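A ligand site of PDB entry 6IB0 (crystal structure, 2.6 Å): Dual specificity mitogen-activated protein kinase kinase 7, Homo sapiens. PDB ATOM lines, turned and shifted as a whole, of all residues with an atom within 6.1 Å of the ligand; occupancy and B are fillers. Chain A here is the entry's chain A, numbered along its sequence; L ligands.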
ATOM      1  N   MET A  36     -23.337 -16.120  21.869  1.00  0.00           N
ATOM      2  CA  MET A  36     -24.029 -14.948  21.319  1.00  0.00           C
ATOM      3  C   MET A  36     -23.313 -13.673  21.770  1.00  0.00           C
ATOM      4  O   MET A  36     -23.780 -12.934  22.637  1.00  0.00           O
ATOM      5  CB  MET A  36     -25.493 -14.947  21.736  1.00  0.00           C
ATOM      6  CG  MET A  36     -26.163 -16.306  21.687  1.00  0.00           C
ATOM      7  SD  MET A  36     -27.837 -16.302  22.368  1.00  0.00           S
ATOM      8  CE  MET A  36     -28.697 -15.264  21.195  1.00  0.00           C
ATOM      9  N   GLY A  37     -22.160 -13.433  21.152  1.00  0.00           N
ATOM     10  CA  GLY A  37     -21.345 -12.298  21.506  1.00  0.00           C
ATOM     11  C   GLY A  37     -20.648 -12.468  22.840  1.00  0.00           C
ATOM     12  O   GLY A  37     -21.044 -13.247  23.702  1.00  0.00           O
ATOM     13  N   SER A  38     -19.570 -11.696  23.012  1.00  0.00           N
ATOM     14  CA  SER A  38     -18.801 -11.746  24.253  1.00  0.00           C
ATOM     15  C   SER A  38     -19.644 -11.158  25.379  1.00  0.00           C
ATOM     16  O   SER A  38     -19.869  -9.943  25.428  1.00  0.00           O
ATOM     17  CB  SER A  38     -17.487 -10.991  24.095  1.00  0.00           C
ATOM     18  OG  SER A  38     -16.836 -10.865  25.342  1.00  0.00           O
ATOM     19  N   GLY A  39     -20.100 -12.018  26.291  1.00  0.00           N
ATOM     20  CA  GLY A  39     -20.950 -11.547  27.369  1.00  0.00           C
ATOM     21  C   GLY A  39     -20.192 -10.659  28.338  1.00  0.00           C
ATOM     22  O   GLY A  39     -19.021 -10.892  28.643  1.00  0.00           O
ATOM     23  N   THR A  40     -20.871  -9.614  28.813  1.00  0.00           N
ATOM     24  CA  THR A  40     -20.331  -8.724  29.835  1.00  0.00           C
ATOM     25  C   THR A  40     -20.853  -9.050  31.221  1.00  0.00           C
ATOM     26  O   THR A  40     -20.334  -8.508  32.206  1.00  0.00           O
ATOM     27  CB  THR A  40     -20.647  -7.264  29.486  1.00  0.00           C
ATOM     28  OG1 THR A  40     -22.063  -7.046  29.612  1.00  0.00           O
ATOM     29  CG2 THR A  40     -20.218  -6.959  28.067  1.00  0.00           C
ATOM     30  N   GLY A  42     -21.450 -12.618  31.943  1.00  0.00           N
ATOM     31  CA  GLY A  42     -21.459 -14.051  31.751  1.00  0.00           C
ATOM     32  C   GLY A  42     -21.466 -14.486  30.298  1.00  0.00           C
ATOM     33  O   GLY A  42     -22.128 -13.878  29.447  1.00  0.00           O
ATOM     34  N   VAL A  44     -22.662 -16.333  27.203  1.00  0.00           N
ATOM     35  CA  VAL A  44     -24.019 -16.720  26.819  1.00  0.00           C
ATOM     36  C   VAL A  44     -23.952 -17.586  25.566  1.00  0.00           C
ATOM     37  O   VAL A  44     -23.398 -17.167  24.547  1.00  0.00           O
ATOM     38  CB  VAL A  44     -24.920 -15.491  26.581  1.00  0.00           C
ATOM     39  CG1 VAL A  44     -26.196 -15.904  25.864  1.00  0.00           C
ATOM     40  CG2 VAL A  44     -25.235 -14.803  27.898  1.00  0.00           C
ATOM     41  N   ALA A  57     -31.397 -19.436  25.177  1.00  0.00           N
ATOM     42  CA  ALA A  57     -30.121 -18.864  25.610  1.00  0.00           C
ATOM     43  C   ALA A  57     -29.760 -19.482  26.951  1.00  0.00           C
ATOM     44  O   ALA A  57     -30.629 -19.748  27.784  1.00  0.00           O
ATOM     45  CB  ALA A  57     -30.216 -17.343  25.738  1.00  0.00           C
ATOM     46  N   LYS A  59     -26.744 -19.043  29.950  1.00  0.00           N
ATOM     47  CA  LYS A  59     -25.577 -18.389  30.524  1.00  0.00           C
ATOM     48  C   LYS A  59     -24.794 -19.375  31.383  1.00  0.00           C
ATOM     49  O   LYS A  59     -25.379 -20.199  32.082  1.00  0.00           O
ATOM     50  CB  LYS A  59     -26.000 -17.176  31.357  1.00  0.00           C
ATOM     51  CG  LYS A  59     -24.857 -16.476  32.085  1.00  0.00           C
ATOM     52  CD  LYS A  59     -25.402 -15.380  32.983  1.00  0.00           C
ATOM     53  CE  LYS A  59     -26.227 -14.380  32.191  1.00  0.00           C
ATOM     54  NZ  LYS A  59     -26.414 -13.107  32.923  1.00  0.00           N
ATOM     55  N   ASP A  76     -27.647 -10.500  38.990  1.00  0.00           N
ATOM     56  CA  ASP A  76     -28.663 -10.462  37.938  1.00  0.00           C
ATOM     57  C   ASP A  76     -29.607 -11.643  38.061  1.00  0.00           C
ATOM     58  O   ASP A  76     -30.829 -11.507  37.843  1.00  0.00           O
ATOM     59  CB  ASP A  76     -28.006 -10.445  36.557  1.00  0.00           C
ATOM     60  CG  ASP A  76     -28.990 -10.708  35.432  1.00  0.00           C
ATOM     61  OD1 ASP A  76     -29.414 -11.874  35.270  1.00  0.00           O
ATOM     62  OD2 ASP A  76     -29.351  -9.753  34.702  1.00  0.00           O
ATOM     63  N   VAL A  90     -36.447  -9.988  30.583  1.00  0.00           N
ATOM     64  CA  VAL A  90     -36.027 -11.268  30.014  1.00  0.00           C
ATOM     65  C   VAL A  90     -36.318 -12.369  31.018  1.00  0.00           C
ATOM     66  O   VAL A  90     -35.789 -12.354  32.139  1.00  0.00           O
ATOM     67  CB  VAL A  90     -34.541 -11.255  29.625  1.00  0.00           C
ATOM     68  CG1 VAL A  90     -34.256 -12.333  28.605  1.00  0.00           C
ATOM     69  CG2 VAL A  90     -34.154  -9.882  29.091  1.00  0.00           C
ATOM     70  N   MET A 106     -32.201 -18.934  29.832  1.00  0.00           N
ATOM     71  CA  MET A 106     -32.968 -17.725  29.569  1.00  0.00           C
ATOM     72  C   MET A 106     -33.769 -17.862  28.283  1.00  0.00           C
ATOM     73  O   MET A 106     -33.417 -18.611  27.363  1.00  0.00           O
ATOM     74  CB  MET A 106     -32.046 -16.498  29.450  1.00  0.00           C
ATOM     75  CG  MET A 106     -31.250 -16.171  30.706  1.00  0.00           C
ATOM     76  SD  MET A 106     -32.310 -15.616  32.062  1.00  0.00           S
ATOM     77  CE  MET A 106     -33.297 -14.361  31.242  1.00  0.00           C
ATOM     78  N   GLU A 107     -34.872 -17.116  28.228  1.00  0.00           N
ATOM     79  CA  GLU A 107     -35.635 -16.979  26.996  1.00  0.00           C
ATOM     80  C   GLU A 107     -34.762 -16.363  25.909  1.00  0.00           C
ATOM     81  O   GLU A 107     -34.054 -15.379  26.153  1.00  0.00           O
ATOM     82  CB  GLU A 107     -36.877 -16.129  27.265  1.00  0.00           C
ATOM     83  CG  GLU A 107     -37.279 -15.128  26.199  1.00  0.00           C
ATOM     84  CD  GLU A 107     -38.663 -14.558  26.471  1.00  0.00           C
ATOM     85  OE1 GLU A 107     -38.928 -14.128  27.619  1.00  0.00           O
ATOM     86  OE2 GLU A 107     -39.504 -14.557  25.545  1.00  0.00           O
ATOM     87  N   LEU A 108     -34.785 -16.958  24.716  1.00  0.00           N
ATOM     88  CA  LEU A 108     -33.892 -16.560  23.645  1.00  0.00           C
ATOM     89  C   LEU A 108     -34.407 -15.289  22.979  1.00  0.00           C
ATOM     90  O   LEU A 108     -35.524 -15.259  22.450  1.00  0.00           O
ATOM     91  CB  LEU A 108     -33.755 -17.683  22.611  1.00  0.00           C
ATOM     92  CG  LEU A 108     -32.982 -17.324  21.333  1.00  0.00           C
ATOM     93  CD1 LEU A 108     -31.505 -17.093  21.631  1.00  0.00           C
ATOM     94  CD2 LEU A 108     -33.153 -18.381  20.254  1.00  0.00           C
ATOM     95  N   MET A 109     -33.595 -14.234  23.004  1.00  0.00           N
ATOM     96  CA  MET A 109     -33.944 -12.956  22.418  1.00  0.00           C
ATOM     97  C   MET A 109     -33.104 -12.704  21.169  1.00  0.00           C
ATOM     98  O   MET A 109     -32.085 -13.368  20.938  1.00  0.00           O
ATOM     99  CB  MET A 109     -33.750 -11.820  23.435  1.00  0.00           C
ATOM    100  CG  MET A 109     -34.666 -11.907  24.648  1.00  0.00           C
ATOM    101  SD  MET A 109     -36.355 -11.406  24.263  1.00  0.00           S
ATOM    102  CE  MET A 109     -36.101  -9.699  23.804  1.00  0.00           C
ATOM    103  N   GLY A 110     -33.545 -11.742  20.372  1.00  0.00           N
ATOM    104  CA  GLY A 110     -32.898 -11.449  19.109  1.00  0.00           C
ATOM    105  C   GLY A 110     -31.565 -10.730  19.241  1.00  0.00           C
ATOM    106  O   GLY A 110     -30.528 -11.256  18.817  1.00  0.00           O
ATOM    107  N   THR A 111     -31.564  -9.543  19.835  1.00  0.00           N
ATOM    108  CA  THR A 111     -30.355  -8.742  19.932  1.00  0.00           C
ATOM    109  C   THR A 111     -30.658  -7.497  20.763  1.00  0.00           C
ATOM    110  O   THR A 111     -31.806  -7.231  21.110  1.00  0.00           O
ATOM    111  CB  THR A 111     -29.835  -8.341  18.551  1.00  0.00           C
ATOM    112  OG1 THR A 111     -28.660  -7.539  18.686  1.00  0.00           O
ATOM    113  CG2 THR A 111     -30.901  -7.554  17.786  1.00  0.00           C
ATOM    114  N   CYS A 112     -29.610  -6.750  21.081  1.00  0.00           N
ATOM    115  CA  CYS A 112     -29.770  -5.483  21.779  1.00  0.00           C
ATOM    116  C   CYS A 112     -30.101  -4.368  20.789  1.00  0.00           C
ATOM    117  O   CYS A 112     -29.951  -4.508  19.575  1.00  0.00           O
ATOM    118  CB  CYS A 112     -28.537  -5.148  22.595  1.00  0.00           C
ATOM    119  SG  CYS A 112     -27.027  -4.964  21.623  1.00  0.00           S
ATOM    120  N   ALA A 113     -30.596  -3.258  21.338  1.00  0.00           N
ATOM    121  CA  ALA A 113     -30.865  -2.066  20.539  1.00  0.00           C
ATOM    122  C   ALA A 113     -29.588  -1.360  20.130  1.00  0.00           C
ATOM    123  O   ALA A 113     -29.578  -0.642  19.120  1.00  0.00           O
ATOM    124  CB  ALA A 113     -31.786  -1.139  21.321  1.00  0.00           C
ATOM    125  N   GLU A 114     -28.494  -1.534  20.881  1.00  0.00           N
ATOM    126  CA  GLU A 114     -27.221  -0.944  20.472  1.00  0.00           C
ATOM    127  C   GLU A 114     -26.693  -1.602  19.204  1.00  0.00           C
ATOM    128  O   GLU A 114     -26.219  -0.921  18.290  1.00  0.00           O
ATOM    129  CB  GLU A 114     -26.194  -1.043  21.596  1.00  0.00           C
ATOM    130  CG  GLU A 114     -24.884  -0.327  21.292  1.00  0.00           C
ATOM    131  CD  GLU A 114     -23.669  -1.146  21.664  1.00  0.00           C
ATOM    132  OE1 GLU A 114     -23.574  -2.309  21.201  1.00  0.00           O
ATOM    133  OE2 GLU A 114     -22.803  -0.649  22.425  1.00  0.00           O
ATOM    134  N   LYS A 115     -26.741  -2.940  19.141  1.00  0.00           N
ATOM    135  CA  LYS A 115     -26.367  -3.630  17.912  1.00  0.00           C
ATOM    136  C   LYS A 115     -27.416  -3.443  16.824  1.00  0.00           C
ATOM    137  O   LYS A 115     -27.084  -3.462  15.639  1.00  0.00           O
ATOM    138  CB  LYS A 115     -26.130  -5.117  18.195  1.00  0.00           C
ATOM    139  CG  LYS A 115     -24.804  -5.397  18.872  1.00  0.00           C
ATOM    140  CD  LYS A 115     -24.662  -6.848  19.279  1.00  0.00           C
ATOM    141  CE  LYS A 115     -23.269  -7.125  19.840  1.00  0.00           C
ATOM    142  NZ  LYS A 115     -23.172  -8.453  20.494  1.00  0.00           N
ATOM    143  N   PRO A 156     -28.826   1.318  25.629  1.00  0.00           N
ATOM    144  CA  PRO A 156     -29.311   0.563  24.466  1.00  0.00           C
ATOM    145  C   PRO A 156     -28.840  -0.883  24.424  1.00  0.00           C
ATOM    146  O   PRO A 156     -29.546  -1.744  23.898  1.00  0.00           O
ATOM    147  CB  PRO A 156     -28.765   1.358  23.275  1.00  0.00           C
ATOM    148  CG  PRO A 156     -28.644   2.753  23.808  1.00  0.00           C
ATOM    149  CD  PRO A 156     -28.170   2.574  25.215  1.00  0.00           C
ATOM    150  N   SER A 157     -27.639  -1.172  24.946  1.00  0.00           N
ATOM    151  CA  SER A 157     -27.153  -2.551  24.967  1.00  0.00           C
ATOM    152  C   SER A 157     -27.895  -3.421  25.967  1.00  0.00           C
ATOM    153  O   SER A 157     -27.682  -4.640  25.984  1.00  0.00           O
ATOM    154  CB  SER A 157     -25.647  -2.574  25.269  1.00  0.00           C
ATOM    155  OG  SER A 157     -25.343  -1.750  26.383  1.00  0.00           O
ATOM    156  N   LEU A 160     -33.269  -5.653  24.874  1.00  0.00           N
ATOM    157  CA  LEU A 160     -33.269  -6.770  23.951  1.00  0.00           C
ATOM    158  C   LEU A 160     -34.578  -6.833  23.171  1.00  0.00           C
ATOM    159  O   LEU A 160     -35.646  -6.599  23.728  1.00  0.00           O
ATOM    160  CB  LEU A 160     -33.034  -8.086  24.694  1.00  0.00           C
ATOM    161  CG  LEU A 160     -31.735  -8.201  25.497  1.00  0.00           C
ATOM    162  CD1 LEU A 160     -31.487  -9.643  25.921  1.00  0.00           C
ATOM    163  CD2 LEU A 160     -30.559  -7.654  24.709  1.00  0.00           C
ATOM    164  N   CYS A 170     -32.640  -6.123  30.516  1.00  0.00           N
ATOM    165  CA  CYS A 170     -31.770  -7.214  30.951  1.00  0.00           C
ATOM    166  C   CYS A 170     -30.573  -6.668  31.719  1.00  0.00           C
ATOM    167  O   CYS A 170     -30.345  -5.452  31.785  1.00  0.00           O
ATOM    168  CB  CYS A 170     -31.306  -8.050  29.757  1.00  0.00           C
ATOM    169  SG  CYS A 170     -30.017  -7.277  28.744  1.00  0.00           S
ATOM    170  N   ASP A 171     -29.815  -7.589  32.316  1.00  0.00           N
ATOM    171  CA  ASP A 171     -28.531  -7.323  32.943  1.00  0.00           C
ATOM    172  C   ASP A 171     -28.684  -6.425  34.173  1.00  0.00           C
ATOM    173  O   ASP A 171     -28.351  -5.238  34.183  1.00  0.00           O
ATOM    174  CB  ASP A 171     -27.534  -6.706  31.955  1.00  0.00           C
ATOM    175  CG  ASP A 171     -26.114  -6.694  32.484  1.00  0.00           C
ATOM    176  OD1 ASP A 171     -25.906  -7.125  33.635  1.00  0.00           O
ATOM    177  OD2 ASP A 171     -25.203  -6.239  31.757  1.00  0.00           O
HETATM  178  N1  LIG L   1     -31.225 -13.587  24.377  1.00  0.00           N
HETATM  179  C1  LIG L   1     -30.351 -13.224  23.344  1.00  0.00           C
HETATM  180  C2  LIG L   1     -29.650 -12.827  25.918  1.00  0.00           C
HETATM  181  C3  LIG L   1     -30.829 -13.374  25.639  1.00  0.00           C
HETATM  182  C4  LIG L   1     -28.810 -12.439  24.955  1.00  0.00           C
HETATM  183  C5  LIG L   1     -29.022 -12.509  27.045  1.00  0.00           C
HETATM  184  C6  LIG L   1     -29.513 -12.697  28.389  1.00  0.00           C
HETATM  185  C7  LIG L   1     -29.907 -12.849  29.504  1.00  0.00           C
HETATM  186  C8  LIG L   1     -26.424 -11.371  25.078  1.00  0.00           C
HETATM  187  C9  LIG L   1     -25.190 -11.635  25.946  1.00  0.00           C
HETATM  188  C10 LIG L   1     -24.021 -10.924  25.271  1.00  0.00           C
HETATM  189  C11 LIG L   1     -24.223  -9.442  25.143  1.00  0.00           C
HETATM  190  C12 LIG L   1     -26.654  -9.854  24.798  1.00  0.00           C
HETATM  191  C13 LIG L   1     -25.376  -8.090  23.536  1.00  0.00           C
HETATM  192  C14 LIG L   1     -26.603  -7.772  22.703  1.00  0.00           C
HETATM  193  C15 LIG L   1     -26.449  -6.322  22.228  1.00  0.00           C
HETATM  194  N2  LIG L   1     -29.121 -12.645  23.673  1.00  0.00           N
HETATM  195  N3  LIG L   1     -31.605 -13.694  26.675  1.00  0.00           N
HETATM  196  N4  LIG L   1     -27.695 -11.988  25.545  1.00  0.00           N
HETATM  197  N5  LIG L   1     -27.842 -11.981  26.748  1.00  0.00           N
HETATM  198  N6  LIG L   1     -25.427  -9.163  24.339  1.00  0.00           N
HETATM  199  O1  LIG L   1     -24.309  -7.535  23.259  1.00  0.00           O
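The side-chain sulfur of Cys 112 is covalently linked to a carbon (C15) of the ligand (1.6 Å).
A nitrogen (N1) of the ligand sits at hydrogen-bond distance from the backbone NH (N) of Met 109 (2.8 Å).
The backbone carbonyl oxygen of Glu 107 sits at hydrogen-bond distance from a nitrogen (N3) of the ligand, at 3.0 Å.
An oxygen (O1) of the ligand lies within hydrogen-bond range of the side-chain amino group of Lys 115, 3.1 Å away.
Residues that only touch the ligand: Met 36 (3.3 Å), Val 90 (3.6 Å), Leu 160 (3.7 Å), Val 44 (3.7 Å), Gly 39 (3.8 Å), Met 106 (3.8 Å) and Leu 108 (3.9 Å).
Hydrophobic or aromatic side chains within 4 Å of the ligand: Met 36, Val 44, Val 90, Met 106, Met 109 and Leu 160.
Within 4 Å of the ligand: Met 36, Gly 39, Val 44, Val 90, Met 106, Glu 107, Leu 108, Met 109, Cys 112, Lys 115 and Leu 160.
The side-chain sulfur (SG) of Cys 112 sits at hydrogen-bond distance from the backbone NH (N) of Lys 115 (3.2 Å).
The backbone NH (N) of Met 36 is in hydrogen-bond range of the backbone carbonyl oxygen (O) of Val 44.
The backbone carbonyl oxygen (O) of Ala 57 sits at hydrogen-bond distance from the backbone NH (N) of Met 106 (2.7 Å).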
